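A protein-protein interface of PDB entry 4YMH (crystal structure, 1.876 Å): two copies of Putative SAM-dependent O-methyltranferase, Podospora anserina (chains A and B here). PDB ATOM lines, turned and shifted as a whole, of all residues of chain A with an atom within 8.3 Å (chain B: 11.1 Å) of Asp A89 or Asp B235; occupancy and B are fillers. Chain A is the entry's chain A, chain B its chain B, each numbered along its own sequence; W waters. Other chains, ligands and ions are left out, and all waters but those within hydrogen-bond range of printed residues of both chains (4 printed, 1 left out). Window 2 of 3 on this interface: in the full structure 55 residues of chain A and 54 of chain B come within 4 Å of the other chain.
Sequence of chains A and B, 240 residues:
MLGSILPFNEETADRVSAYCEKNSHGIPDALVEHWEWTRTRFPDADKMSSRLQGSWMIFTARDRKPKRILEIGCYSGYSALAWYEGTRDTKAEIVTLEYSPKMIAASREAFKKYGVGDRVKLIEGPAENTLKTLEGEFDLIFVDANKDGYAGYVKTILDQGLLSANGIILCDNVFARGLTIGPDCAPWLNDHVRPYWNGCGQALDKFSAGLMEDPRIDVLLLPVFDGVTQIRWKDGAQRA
OD2 of Asp A63 lies within salt-bridge range of NH1 of Arg B64, 2.7 Å away. The side-chain amino group (NZ) of Lys A65 sits at hydrogen-bond distance from the side-chain amide oxygen (OD1) of Asn B166 (3.2 Å). The backbone carbonyl oxygen of Arg A62 is in hydrogen-bond range of the guanidinium group of Arg B232.
The backbone carbonyl oxygen (O) of Asn B166 lies within hydrogen-bond range of the guanidinium group (NH2) of Arg B64 (3.5 Å). The guanidinium group of Arg B232 lies within salt-bridge range of the side-chain carboxylate of Asp B235 (2.7 Å). NZ of Lys A65 is in hydrogen-bond range of O of Arg A62, at 3.3 Å. OD2 of Asp B218 lies within salt-bridge range of NH1 of Arg B232, at 2.8 Å. O of Asp A63 is in hydrogen-bond range of NZ of Lys A65 (2.8 Å).
CE2 of Phe A59 touches O of Asp B218, at 3.6 Å. Arg B232 touches Phe A59 (CG to CE2, 3.8 Å). OD2 of Asp B235 touches CD of Arg A62, at 3.7 Å. Arg B232 touches Asp A63 (NE to CA, 3.7 Å). Arg B232 touches Lys A65 (NH2 to NZ, 3.96 Å). OD2 of Asp A89 touches CB of Asp B235 (3.8 Å).
Of the printed residues of chain B, Lys A65 touches Asn B166 and Arg B232. No residue of chain B comes within 4 Å of Thr A87. Asp A89 touches just one residue of chain B: Asp B235. No residue of chain B comes within 4 Å of Thr A90. No residue of chain B comes within 4 Å of Lys A91. Of the printed residues of chain A, Arg B64 touches Asp A63 (2.7 Å). Printed residues of chain A within 4 Å of Asn B166: Lys A65 (3.2 Å). Ile B217 touches none of the printed residues of chain A. Lys B234 touches none of the printed residues of chain A. Asp B235 touches two residues of chain A. The nearest residue of chain B that does not touch Asp A89 is Gly B236 (5.5 Å).
Hydrophobic or aromatic side chains of chain A that line the printed part of chain B: Phe A59. Among the printed residues, 9 pairs touch across the chains.
No position is printed for both chains.
Water W1 lies within hydrogen-bond range of OD1 of Asp A63 (2.6 Å), NE of Arg B232 (3.0 Å) and O of Gly B167 (3.2 Å). Water W2 lies within hydrogen-bond range of the backbone carbonyl oxygen (O) of Asn B166 (2.6 Å) and the backbone carbonyl oxygen (O) of Asp A63 (2.9 Å). Water W3 lies within hydrogen-bond range of O of Arg A62 and OD2 of Asp B235. Water W4 lies within hydrogen-bond range of the side-chain carboxylate (OD1) of Asp B218 (2.7 Å) and the guanidinium group (NH1) of Arg A62 (3.3 Å).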
ATOM      1  N   ILE A  58      28.675 -31.950 -29.074  1.00  0.00           N
ATOM      2  CA  ILE A  58      28.014 -32.032 -27.779  1.00  0.00           C
ATOM      3  C   ILE A  58      26.878 -31.000 -27.672  1.00  0.00           C
ATOM      4  O   ILE A  58      25.778 -31.317 -27.207  1.00  0.00           O
ATOM      5  CB  ILE A  58      29.021 -31.836 -26.627  1.00  0.00           C
ATOM      6  CG1 ILE A  58      30.029 -33.004 -26.628  1.00  0.00           C
ATOM      7  CG2 ILE A  58      28.292 -31.754 -25.294  1.00  0.00           C
ATOM      8  CD1 ILE A  58      31.098 -32.900 -25.573  1.00  0.00           C
ATOM      9  N   PHE A  59      27.155 -29.774 -28.108  1.00  0.00           N
ATOM     10  CA  PHE A  59      26.134 -28.716 -28.110  1.00  0.00           C
ATOM     11  C   PHE A  59      24.925 -29.138 -28.936  1.00  0.00           C
ATOM     12  O   PHE A  59      23.773 -29.038 -28.491  1.00  0.00           O
ATOM     13  CB  PHE A  59      26.714 -27.403 -28.652  1.00  0.00           C
ATOM     14  CG  PHE A  59      25.759 -26.217 -28.568  1.00  0.00           C
ATOM     15  CD1 PHE A  59      24.751 -26.041 -29.503  1.00  0.00           C
ATOM     16  CD2 PHE A  59      25.893 -25.271 -27.551  1.00  0.00           C
ATOM     17  CE1 PHE A  59      23.882 -24.946 -29.424  1.00  0.00           C
ATOM     18  CE2 PHE A  59      25.046 -24.175 -27.478  1.00  0.00           C
ATOM     19  CZ  PHE A  59      24.028 -24.021 -28.397  1.00  0.00           C
ATOM     20  N   ALA A  61      23.932 -32.123 -29.852  1.00  0.00           N
ATOM     21  CA  ALA A  61      23.193 -33.196 -29.188  1.00  0.00           C
ATOM     22  C   ALA A  61      22.357 -32.711 -27.993  1.00  0.00           C
ATOM     23  O   ALA A  61      21.231 -33.167 -27.802  1.00  0.00           O
ATOM     24  CB  ALA A  61      24.150 -34.286 -28.729  1.00  0.00           C
ATOM     25  N   ARG A  62      22.903 -31.820 -27.174  1.00  0.00           N
ATOM     26  CA  ARG A  62      22.131 -31.317 -26.036  1.00  0.00           C
ATOM     27  C   ARG A  62      20.941 -30.493 -26.508  1.00  0.00           C
ATOM     28  O   ARG A  62      19.872 -30.492 -25.893  1.00  0.00           O
ATOM     29  CB  ARG A  62      23.011 -30.482 -25.098  1.00  0.00           C
ATOM     30  CG  ARG A  62      24.054 -31.335 -24.352  1.00  0.00           C
ATOM     31  CD  ARG A  62      24.499 -30.705 -23.058  1.00  0.00           C
ATOM     32  NE  ARG A  62      25.476 -31.547 -22.368  1.00  0.00           N
ATOM     33  CZ  ARG A  62      26.730 -31.190 -22.098  1.00  0.00           C
ATOM     34  NH1 ARG A  62      27.169 -29.981 -22.424  1.00  0.00           N
ATOM     35  NH2 ARG A  62      27.539 -32.038 -21.471  1.00  0.00           N
ATOM     36  N   ASP A  63      21.143 -29.785 -27.605  1.00  0.00           N
ATOM     37  CA  ASP A  63      20.121 -28.905 -28.165  1.00  0.00           C
ATOM     38  C   ASP A  63      18.984 -29.701 -28.801  1.00  0.00           C
ATOM     39  O   ASP A  63      17.818 -29.519 -28.445  1.00  0.00           O
ATOM     40  CB  ASP A  63      20.771 -27.964 -29.189  1.00  0.00           C
ATOM     41  CG  ASP A  63      19.774 -27.059 -29.901  1.00  0.00           C
ATOM     42  OD1 ASP A  63      18.727 -26.703 -29.324  1.00  0.00           O
ATOM     43  OD2 ASP A  63      20.069 -26.684 -31.055  1.00  0.00           O
ATOM     44  N   LYS A  65      18.373 -32.924 -28.711  1.00  0.00           N
ATOM     45  CA  LYS A  65      17.918 -34.057 -27.907  1.00  0.00           C
ATOM     46  C   LYS A  65      17.475 -35.263 -28.752  1.00  0.00           C
ATOM     47  O   LYS A  65      16.353 -35.735 -28.621  1.00  0.00           O
ATOM     48  CB  LYS A  65      16.785 -33.601 -26.971  1.00  0.00           C
ATOM     49  CG  LYS A  65      17.290 -32.657 -25.871  1.00  0.00           C
ATOM     50  CD  LYS A  65      16.188 -32.037 -25.034  1.00  0.00           C
ATOM     51  CE  LYS A  65      15.667 -30.757 -25.678  1.00  0.00           C
ATOM     52  NZ  LYS A  65      16.702 -29.685 -25.857  1.00  0.00           N
ATOM     53  N   TRP A  83      29.035 -37.629 -28.859  1.00  0.00           N
ATOM     54  CA  TRP A  83      27.584 -37.861 -28.866  1.00  0.00           C
ATOM     55  C   TRP A  83      27.102 -38.424 -27.530  1.00  0.00           C
ATOM     56  O   TRP A  83      26.051 -38.027 -26.990  1.00  0.00           O
ATOM     57  CB  TRP A  83      27.190 -38.826 -30.001  1.00  0.00           C
ATOM     58  CG  TRP A  83      27.565 -38.372 -31.394  1.00  0.00           C
ATOM     59  CD1 TRP A  83      28.261 -39.091 -32.327  1.00  0.00           C
ATOM     60  CD2 TRP A  83      27.260 -37.113 -32.009  1.00  0.00           C
ATOM     61  NE1 TRP A  83      28.414 -38.355 -33.476  1.00  0.00           N
ATOM     62  CE2 TRP A  83      27.809 -37.138 -33.307  1.00  0.00           C
ATOM     63  CE3 TRP A  83      26.576 -35.964 -31.587  1.00  0.00           C
ATOM     64  CZ2 TRP A  83      27.697 -36.058 -34.188  1.00  0.00           C
ATOM     65  CZ3 TRP A  83      26.469 -34.899 -32.457  1.00  0.00           C
ATOM     66  CH2 TRP A  83      27.024 -34.953 -33.749  1.00  0.00           C
ATOM     67  N   TYR A  84      27.878 -39.374 -27.009  1.00  0.00           N
ATOM     68  CA  TYR A  84      27.616 -39.974 -25.705  1.00  0.00           C
ATOM     69  C   TYR A  84      27.515 -38.894 -24.627  1.00  0.00           C
ATOM     70  O   TYR A  84      26.544 -38.854 -23.852  1.00  0.00           O
ATOM     71  CB  TYR A  84      28.715 -41.007 -25.375  1.00  0.00           C
ATOM     72  CG  TYR A  84      28.575 -41.674 -24.014  1.00  0.00           C
ATOM     73  CD1 TYR A  84      27.736 -42.768 -23.835  1.00  0.00           C
ATOM     74  CD2 TYR A  84      29.278 -41.205 -22.916  1.00  0.00           C
ATOM     75  CE1 TYR A  84      27.600 -43.373 -22.597  1.00  0.00           C
ATOM     76  CE2 TYR A  84      29.147 -41.803 -21.662  1.00  0.00           C
ATOM     77  CZ  TYR A  84      28.307 -42.889 -21.511  1.00  0.00           C
ATOM     78  OH  TYR A  84      28.177 -43.491 -20.279  1.00  0.00           O
ATOM     79  N   GLU A  85      28.493 -37.994 -24.596  1.00  0.00           N
ATOM     80  CA  GLU A  85      28.477 -36.920 -23.601  1.00  0.00           C
ATOM     81  C   GLU A  85      27.255 -36.018 -23.786  1.00  0.00           C
ATOM     82  O   GLU A  85      26.658 -35.541 -22.809  1.00  0.00           O
ATOM     83  CB  GLU A  85      29.757 -36.075 -23.683  1.00  0.00           C
ATOM     84  CG  GLU A  85      31.022 -36.742 -23.123  1.00  0.00           C
ATOM     85  CD  GLU A  85      31.033 -36.860 -21.603  1.00  0.00           C
ATOM     86  OE1 GLU A  85      30.099 -36.354 -20.934  1.00  0.00           O
ATOM     87  OE2 GLU A  85      31.995 -37.457 -21.073  1.00  0.00           O
ATOM     88  N   GLY A  86      26.886 -35.788 -25.042  1.00  0.00           N
ATOM     89  CA  GLY A  86      25.780 -34.890 -25.330  1.00  0.00           C
ATOM     90  C   GLY A  86      24.412 -35.488 -25.069  1.00  0.00           C
ATOM     91  O   GLY A  86      23.408 -34.778 -25.114  1.00  0.00           O
ATOM     92  N   THR A  87      24.363 -36.795 -24.812  1.00  0.00           N
ATOM     93  CA  THR A  87      23.085 -37.453 -24.545  1.00  0.00           C
ATOM     94  C   THR A  87      23.015 -38.202 -23.204  1.00  0.00           C
ATOM     95  O   THR A  87      22.237 -39.148 -23.055  1.00  0.00           O
ATOM     96  CB  THR A  87      22.752 -38.441 -25.670  1.00  0.00           C
ATOM     97  OG1 THR A  87      23.834 -39.368 -25.824  1.00  0.00           O
ATOM     98  CG2 THR A  87      22.509 -37.699 -26.976  1.00  0.00           C
ATOM     99  N   ARG A  88      23.808 -37.769 -22.229  1.00  0.00           N
ATOM    100  CA  ARG A  88      23.815 -38.403 -20.916  1.00  0.00           C
ATOM    101  C   ARG A  88      22.448 -38.361 -20.231  1.00  0.00           C
ATOM    102  O   ARG A  88      22.081 -39.293 -19.526  1.00  0.00           O
ATOM    103  CB  ARG A  88      24.848 -37.742 -20.002  1.00  0.00           C
ATOM    104  CG  ARG A  88      26.263 -38.198 -20.226  1.00  0.00           C
ATOM    105  CD  ARG A  88      27.207 -37.575 -19.219  1.00  0.00           C
ATOM    106  NE  ARG A  88      28.585 -37.962 -19.494  1.00  0.00           N
ATOM    107  CZ  ARG A  88      29.178 -39.040 -18.993  1.00  0.00           C
ATOM    108  NH1 ARG A  88      28.517 -39.844 -18.168  1.00  0.00           N
ATOM    109  NH2 ARG A  88      30.436 -39.308 -19.312  1.00  0.00           N
ATOM    110  N   ASP A  89      21.705 -37.281 -20.432  1.00  0.00           N
ATOM    111  CA  ASP A  89      20.442 -37.095 -19.720  1.00  0.00           C
ATOM    112  C   ASP A  89      19.329 -38.007 -20.226  1.00  0.00           C
ATOM    113  O   ASP A  89      18.459 -38.417 -19.460  1.00  0.00           O
ATOM    114  CB  ASP A  89      19.993 -35.633 -19.804  1.00  0.00           C
ATOM    115  CG  ASP A  89      20.725 -34.740 -18.811  1.00  0.00           C
ATOM    116  OD1 ASP A  89      21.378 -35.279 -17.891  1.00  0.00           O
ATOM    117  OD2 ASP A  89      20.638 -33.499 -18.939  1.00  0.00           O
ATOM    118  N   THR A  90      19.361 -38.332 -21.511  1.00  0.00           N
ATOM    119  CA  THR A  90      18.315 -39.149 -22.119  1.00  0.00           C
ATOM    120  C   THR A  90      18.725 -40.602 -22.356  1.00  0.00           C
ATOM    121  O   THR A  90      17.888 -41.442 -22.694  1.00  0.00           O
ATOM    122  CB  THR A  90      17.902 -38.574 -23.460  1.00  0.00           C
ATOM    123  OG1 THR A  90      18.964 -38.790 -24.396  1.00  0.00           O
ATOM    124  CG2 THR A  90      17.640 -37.087 -23.334  1.00  0.00           C
ATOM    125  N   LYS A  91      20.018 -40.880 -22.214  1.00  0.00           N
ATOM    126  CA  LYS A  91      20.572 -42.196 -22.518  1.00  0.00           C
ATOM    127  C   LYS A  91      20.186 -42.642 -23.936  1.00  0.00           C
ATOM    128  O   LYS A  91      19.743 -43.773 -24.145  1.00  0.00           O
ATOM    129  CB  LYS A  91      20.112 -43.224 -21.481  1.00  0.00           C
ATOM    130  CG  LYS A  91      20.317 -42.792 -20.023  1.00  0.00           C
ATOM    131  CD  LYS A  91      21.787 -42.624 -19.661  1.00  0.00           C
ATOM    132  CE  LYS A  91      21.955 -42.123 -18.228  1.00  0.00           C
ATOM    133  NZ  LYS A  91      22.192 -43.220 -17.248  1.00  0.00           N
ATOM    134  N   ALA A  92      20.329 -41.731 -24.897  1.00  0.00           N
ATOM    135  CA  ALA A  92      20.154 -42.058 -26.310  1.00  0.00           C
ATOM    136  C   ALA A  92      21.027 -43.239 -26.725  1.00  0.00           C
ATOM    137  O   ALA A  92      22.173 -43.375 -26.269  1.00  0.00           O
ATOM    138  CB  ALA A  92      20.481 -40.842 -27.192  1.00  0.00           C
ATOM    139  N   ARG A 119      24.384 -48.558 -24.193  1.00  0.00           N
ATOM    140  CA  ARG A 119      23.789 -47.684 -25.218  1.00  0.00           C
ATOM    141  C   ARG A 119      24.700 -47.277 -26.382  1.00  0.00           C
ATOM    142  O   ARG A 119      24.211 -46.747 -27.384  1.00  0.00           O
ATOM    143  CB  ARG A 119      23.217 -46.417 -24.568  1.00  0.00           C
ATOM    144  CG  ARG A 119      24.201 -45.420 -23.971  1.00  0.00           C
ATOM    145  CD  ARG A 119      23.386 -44.329 -23.224  1.00  0.00           C
ATOM    146  NE  ARG A 119      24.197 -43.240 -22.670  1.00  0.00           N
ATOM    147  CZ  ARG A 119      24.441 -42.087 -23.291  1.00  0.00           C
ATOM    148  NH1 ARG A 119      23.947 -41.861 -24.495  1.00  0.00           N
ATOM    149  NH2 ARG A 119      25.184 -41.158 -22.709  1.00  0.00           N
ATOM    150  N   ARG B  64      13.990 -26.338 -37.078  1.00  0.00           N
ATOM    151  CA  ARG B  64      13.674 -26.154 -35.659  1.00  0.00           C
ATOM    152  C   ARG B  64      12.189 -25.938 -35.378  1.00  0.00           C
ATOM    153  O   ARG B  64      11.725 -26.194 -34.267  1.00  0.00           O
ATOM    154  CB  ARG B  64      14.464 -24.975 -35.097  1.00  0.00           C
ATOM    155  CG  ARG B  64      15.968 -25.120 -35.224  1.00  0.00           C
ATOM    156  CD  ARG B  64      16.688 -24.011 -34.444  1.00  0.00           C
ATOM    157  NE  ARG B  64      16.443 -24.139 -33.010  1.00  0.00           N
ATOM    158  CZ  ARG B  64      17.223 -24.835 -32.186  1.00  0.00           C
ATOM    159  NH1 ARG B  64      18.304 -25.445 -32.658  1.00  0.00           N
ATOM    160  NH2 ARG B  64      16.923 -24.934 -30.898  1.00  0.00           N
ATOM    161  N   LEU B 163      13.775 -16.316 -23.680  1.00  0.00           N
ATOM    162  CA  LEU B 163      14.191 -17.510 -24.399  1.00  0.00           C
ATOM    163  C   LEU B 163      13.488 -18.732 -23.813  1.00  0.00           C
ATOM    164  O   LEU B 163      13.592 -19.001 -22.613  1.00  0.00           O
ATOM    165  CB  LEU B 163      15.719 -17.690 -24.319  1.00  0.00           C
ATOM    166  CG  LEU B 163      16.317 -18.910 -25.033  1.00  0.00           C
ATOM    167  CD1 LEU B 163      16.218 -18.750 -26.559  1.00  0.00           C
ATOM    168  CD2 LEU B 163      17.765 -19.118 -24.622  1.00  0.00           C
ATOM    169  N   SER B 164      12.779 -19.479 -24.652  1.00  0.00           N
ATOM    170  CA  SER B 164      12.075 -20.674 -24.170  1.00  0.00           C
ATOM    171  C   SER B 164      13.062 -21.759 -23.757  1.00  0.00           C
ATOM    172  O   SER B 164      14.229 -21.722 -24.151  1.00  0.00           O
ATOM    173  CB  SER B 164      11.137 -21.220 -25.241  1.00  0.00           C
ATOM    174  OG  SER B 164      11.892 -21.722 -26.334  1.00  0.00           O
ATOM    175  N   ALA B 165      12.576 -22.738 -22.994  1.00  0.00           N
ATOM    176  CA  ALA B 165      13.413 -23.819 -22.460  1.00  0.00           C
ATOM    177  C   ALA B 165      14.261 -24.528 -23.511  1.00  0.00           C
ATOM    178  O   ALA B 165      15.439 -24.800 -23.277  1.00  0.00           O
ATOM    179  CB  ALA B 165      12.532 -24.845 -21.718  1.00  0.00           C
ATOM    180  N   ASN B 166      13.668 -24.836 -24.661  1.00  0.00           N
ATOM    181  CA  ASN B 166      14.392 -25.541 -25.721  1.00  0.00           C
ATOM    182  C   ASN B 166      14.741 -24.633 -26.885  1.00  0.00           C
ATOM    183  O   ASN B 166      14.990 -25.104 -27.997  1.00  0.00           O
ATOM    184  CB  ASN B 166      13.568 -26.730 -26.212  1.00  0.00           C
ATOM    185  CG  ASN B 166      13.359 -27.774 -25.125  1.00  0.00           C
ATOM    186  OD1 ASN B 166      14.306 -28.175 -24.451  1.00  0.00           O
ATOM    187  ND2 ASN B 166      12.112 -28.183 -24.924  1.00  0.00           N
ATOM    188  N   GLY B 167      14.758 -23.334 -26.614  1.00  0.00           N
ATOM    189  CA  GLY B 167      15.061 -22.342 -27.631  1.00  0.00           C
ATOM    190  C   GLY B 167      16.551 -22.120 -27.843  1.00  0.00           C
ATOM    191  O   GLY B 167      17.389 -22.613 -27.084  1.00  0.00           O
ATOM    192  N   ASP B 214      28.779 -16.920 -17.560  1.00  0.00           N
ATOM    193  CA  ASP B 214      27.375 -17.063 -17.178  1.00  0.00           C
ATOM    194  C   ASP B 214      26.994 -18.528 -17.020  1.00  0.00           C
ATOM    195  O   ASP B 214      26.875 -19.255 -18.016  1.00  0.00           O
ATOM    196  CB  ASP B 214      26.478 -16.407 -18.230  1.00  0.00           C
ATOM    197  CG  ASP B 214      25.029 -16.247 -17.766  1.00  0.00           C
ATOM    198  OD1 ASP B 214      24.581 -17.003 -16.882  1.00  0.00           O
ATOM    199  OD2 ASP B 214      24.336 -15.359 -18.302  1.00  0.00           O
ATOM    200  N   PRO B 215      26.777 -18.964 -15.773  1.00  0.00           N
ATOM    201  CA  PRO B 215      26.482 -20.378 -15.499  1.00  0.00           C
ATOM    202  C   PRO B 215      25.112 -20.842 -15.998  1.00  0.00           C
ATOM    203  O   PRO B 215      24.855 -22.050 -15.973  1.00  0.00           O
ATOM    204  CB  PRO B 215      26.533 -20.462 -13.969  1.00  0.00           C
ATOM    205  CG  PRO B 215      27.250 -19.227 -13.512  1.00  0.00           C
ATOM    206  CD  PRO B 215      26.933 -18.176 -14.532  1.00  0.00           C
ATOM    207  N   ARG B 216      24.243 -19.918 -16.415  1.00  0.00           N
ATOM    208  CA  ARG B 216      22.900 -20.284 -16.897  1.00  0.00           C
ATOM    209  C   ARG B 216      22.849 -20.894 -18.305  1.00  0.00           C
ATOM    210  O   ARG B 216      21.844 -21.506 -18.690  1.00  0.00           O
ATOM    211  CB  ARG B 216      21.990 -19.051 -16.877  1.00  0.00           C
ATOM    212  CG  ARG B 216      21.779 -18.472 -15.486  1.00  0.00           C
ATOM    213  CD  ARG B 216      20.992 -17.156 -15.573  1.00  0.00           C
ATOM    214  NE  ARG B 216      21.732 -16.145 -16.334  1.00  0.00           N
ATOM    215  CZ  ARG B 216      21.310 -14.897 -16.516  1.00  0.00           C
ATOM    216  NH1 ARG B 216      20.150 -14.503 -15.990  1.00  0.00           N
ATOM    217  NH2 ARG B 216      22.044 -14.049 -17.219  1.00  0.00           N
ATOM    218  N   ILE B 217      23.916 -20.729 -19.078  1.00  0.00           N
ATOM    219  CA  ILE B 217      23.837 -21.021 -20.506  1.00  0.00           C
ATOM    220  C   ILE B 217      24.983 -21.925 -21.012  1.00  0.00           C
ATOM    221  O   ILE B 217      26.034 -22.031 -20.363  1.00  0.00           O
ATOM    222  CB  ILE B 217      23.833 -19.711 -21.337  1.00  0.00           C
ATOM    223  CG1 ILE B 217      25.089 -18.898 -21.045  1.00  0.00           C
ATOM    224  CG2 ILE B 217      22.562 -18.891 -21.050  1.00  0.00           C
ATOM    225  CD1 ILE B 217      25.172 -17.564 -21.818  1.00  0.00           C
ATOM    226  N   ASP B 218      24.734 -22.610 -22.129  1.00  0.00           N
ATOM    227  CA  ASP B 218      25.770 -23.285 -22.923  1.00  0.00           C
ATOM    228  C   ASP B 218      26.032 -22.401 -24.130  1.00  0.00           C
ATOM    229  O   ASP B 218      25.084 -21.879 -24.734  1.00  0.00           O
ATOM    230  CB  ASP B 218      25.339 -24.677 -23.407  1.00  0.00           C
ATOM    231  CG  ASP B 218      25.141 -25.676 -22.278  1.00  0.00           C
ATOM    232  OD1 ASP B 218      25.881 -25.625 -21.270  1.00  0.00           O
ATOM    233  OD2 ASP B 218      24.244 -26.538 -22.424  1.00  0.00           O
ATOM    234  N   VAL B 219      27.308 -22.274 -24.509  1.00  0.00           N
ATOM    235  CA  VAL B 219      27.736 -21.314 -25.524  1.00  0.00           C
ATOM    236  C   VAL B 219      28.639 -21.985 -26.553  1.00  0.00           C
ATOM    237  O   VAL B 219      29.552 -22.745 -26.197  1.00  0.00           O
ATOM    238  CB  VAL B 219      28.494 -20.140 -24.891  1.00  0.00           C
ATOM    239  CG1 VAL B 219      28.939 -19.143 -25.967  1.00  0.00           C
ATOM    240  CG2 VAL B 219      27.631 -19.441 -23.819  1.00  0.00           C
ATOM    241  N   ILE B 231      23.589 -19.788 -28.316  1.00  0.00           N
ATOM    242  CA  ILE B 231      23.385 -19.811 -26.870  1.00  0.00           C
ATOM    243  C   ILE B 231      22.128 -20.607 -26.563  1.00  0.00           C
ATOM    244  O   ILE B 231      21.092 -20.413 -27.209  1.00  0.00           O
ATOM    245  CB  ILE B 231      23.225 -18.387 -26.291  1.00  0.00           C
ATOM    246  CG1 ILE B 231      24.390 -17.502 -26.728  1.00  0.00           C
ATOM    247  CG2 ILE B 231      23.097 -18.430 -24.749  1.00  0.00           C
ATOM    248  CD1 ILE B 231      24.211 -16.011 -26.437  1.00  0.00           C
ATOM    249  N   ARG B 232      22.202 -21.485 -25.569  1.00  0.00           N
ATOM    250  CA  ARG B 232      20.987 -22.145 -25.084  1.00  0.00           C
ATOM    251  C   ARG B 232      21.026 -22.191 -23.570  1.00  0.00           C
ATOM    252  O   ARG B 232      22.080 -21.980 -22.976  1.00  0.00           O
ATOM    253  CB  ARG B 232      20.862 -23.565 -25.640  1.00  0.00           C
ATOM    254  CG  ARG B 232      22.018 -24.477 -25.202  1.00  0.00           C
ATOM    255  CD  ARG B 232      21.916 -25.869 -25.809  1.00  0.00           C
ATOM    256  NE  ARG B 232      20.748 -26.589 -25.316  1.00  0.00           N
ATOM    257  CZ  ARG B 232      20.766 -27.373 -24.242  1.00  0.00           C
ATOM    258  NH1 ARG B 232      21.897 -27.541 -23.573  1.00  0.00           N
ATOM    259  NH2 ARG B 232      19.663 -27.996 -23.846  1.00  0.00           N
ATOM    260  N   TRP B 233      19.880 -22.458 -22.951  1.00  0.00           N
ATOM    261  CA  TRP B 233      19.853 -22.678 -21.520  1.00  0.00           C
ATOM    262  C   TRP B 233      20.606 -23.953 -21.156  1.00  0.00           C
ATOM    263  O   TRP B 233      20.438 -24.982 -21.804  1.00  0.00           O
ATOM    264  CB  TRP B 233      18.425 -22.801 -21.016  1.00  0.00           C
ATOM    265  CG  TRP B 233      17.583 -21.559 -21.079  1.00  0.00           C
ATOM    266  CD1 TRP B 233      16.485 -21.361 -21.871  1.00  0.00           C
ATOM    267  CD2 TRP B 233      17.706 -20.384 -20.259  1.00  0.00           C
ATOM    268  NE1 TRP B 233      15.934 -20.125 -21.613  1.00  0.00           N
ATOM    269  CE2 TRP B 233      16.669 -19.503 -20.635  1.00  0.00           C
ATOM    270  CE3 TRP B 233      18.595 -19.986 -19.256  1.00  0.00           C
ATOM    271  CZ2 TRP B 233      16.491 -18.246 -20.033  1.00  0.00           C
ATOM    272  CZ3 TRP B 233      18.422 -18.737 -18.666  1.00  0.00           C
ATOM    273  CH2 TRP B 233      17.376 -17.887 -19.056  1.00  0.00           C
ATOM    274  N   LYS B 234      21.391 -23.902 -20.089  1.00  0.00           N
ATOM    275  CA  LYS B 234      22.039 -25.107 -19.588  1.00  0.00           C
ATOM    276  C   LYS B 234      21.003 -26.065 -19.003  1.00  0.00           C
ATOM    277  O   LYS B 234      20.086 -25.638 -18.302  1.00  0.00           O
ATOM    278  CB  LYS B 234      23.083 -24.753 -18.531  1.00  0.00           C
ATOM    279  CG  LYS B 234      23.599 -25.952 -17.750  1.00  0.00           C
ATOM    280  CD  LYS B 234      24.813 -25.575 -16.925  1.00  0.00           C
ATOM    281  CE  LYS B 234      25.917 -25.007 -17.804  1.00  0.00           C
ATOM    282  NZ  LYS B 234      27.195 -24.862 -17.049  1.00  0.00           N
ATOM    283  N   ASP B 235      21.155 -27.355 -19.288  1.00  0.00           N
ATOM    284  CA  ASP B 235      20.220 -28.378 -18.827  1.00  0.00           C
ATOM    285  C   ASP B 235      20.122 -28.428 -17.300  1.00  0.00           C
ATOM    286  O   ASP B 235      21.123 -28.265 -16.607  1.00  0.00           O
ATOM    287  CB  ASP B 235      20.632 -29.752 -19.363  1.00  0.00           C
ATOM    288  CG  ASP B 235      20.421 -29.875 -20.863  1.00  0.00           C
ATOM    289  OD1 ASP B 235      19.561 -29.145 -21.395  1.00  0.00           O
ATOM    290  OD2 ASP B 235      21.108 -30.698 -21.505  1.00  0.00           O
ATOM    291  N   GLY B 236      18.921 -28.679 -16.783  1.00  0.00           N
ATOM    292  CA  GLY B 236      17.760 -28.966 -17.611  1.00  0.00           C
ATOM    293  C   GLY B 236      16.657 -27.934 -17.502  1.00  0.00           C
ATOM    294  O   GLY B 236      15.686 -27.975 -18.259  1.00  0.00           O
HETATM  295  O   HOH W   1      18.414 -25.615 -27.015  1.00  0.00           O
HETATM  296  O   HOH W   2      15.771 -27.530 -28.581  1.00  0.00           O
HETATM  297  O   HOH W   3      19.479 -31.488 -23.477  1.00  0.00           O
HETATM  298  O   HOH W   4      26.073 -28.027 -19.959  1.00  0.00           O
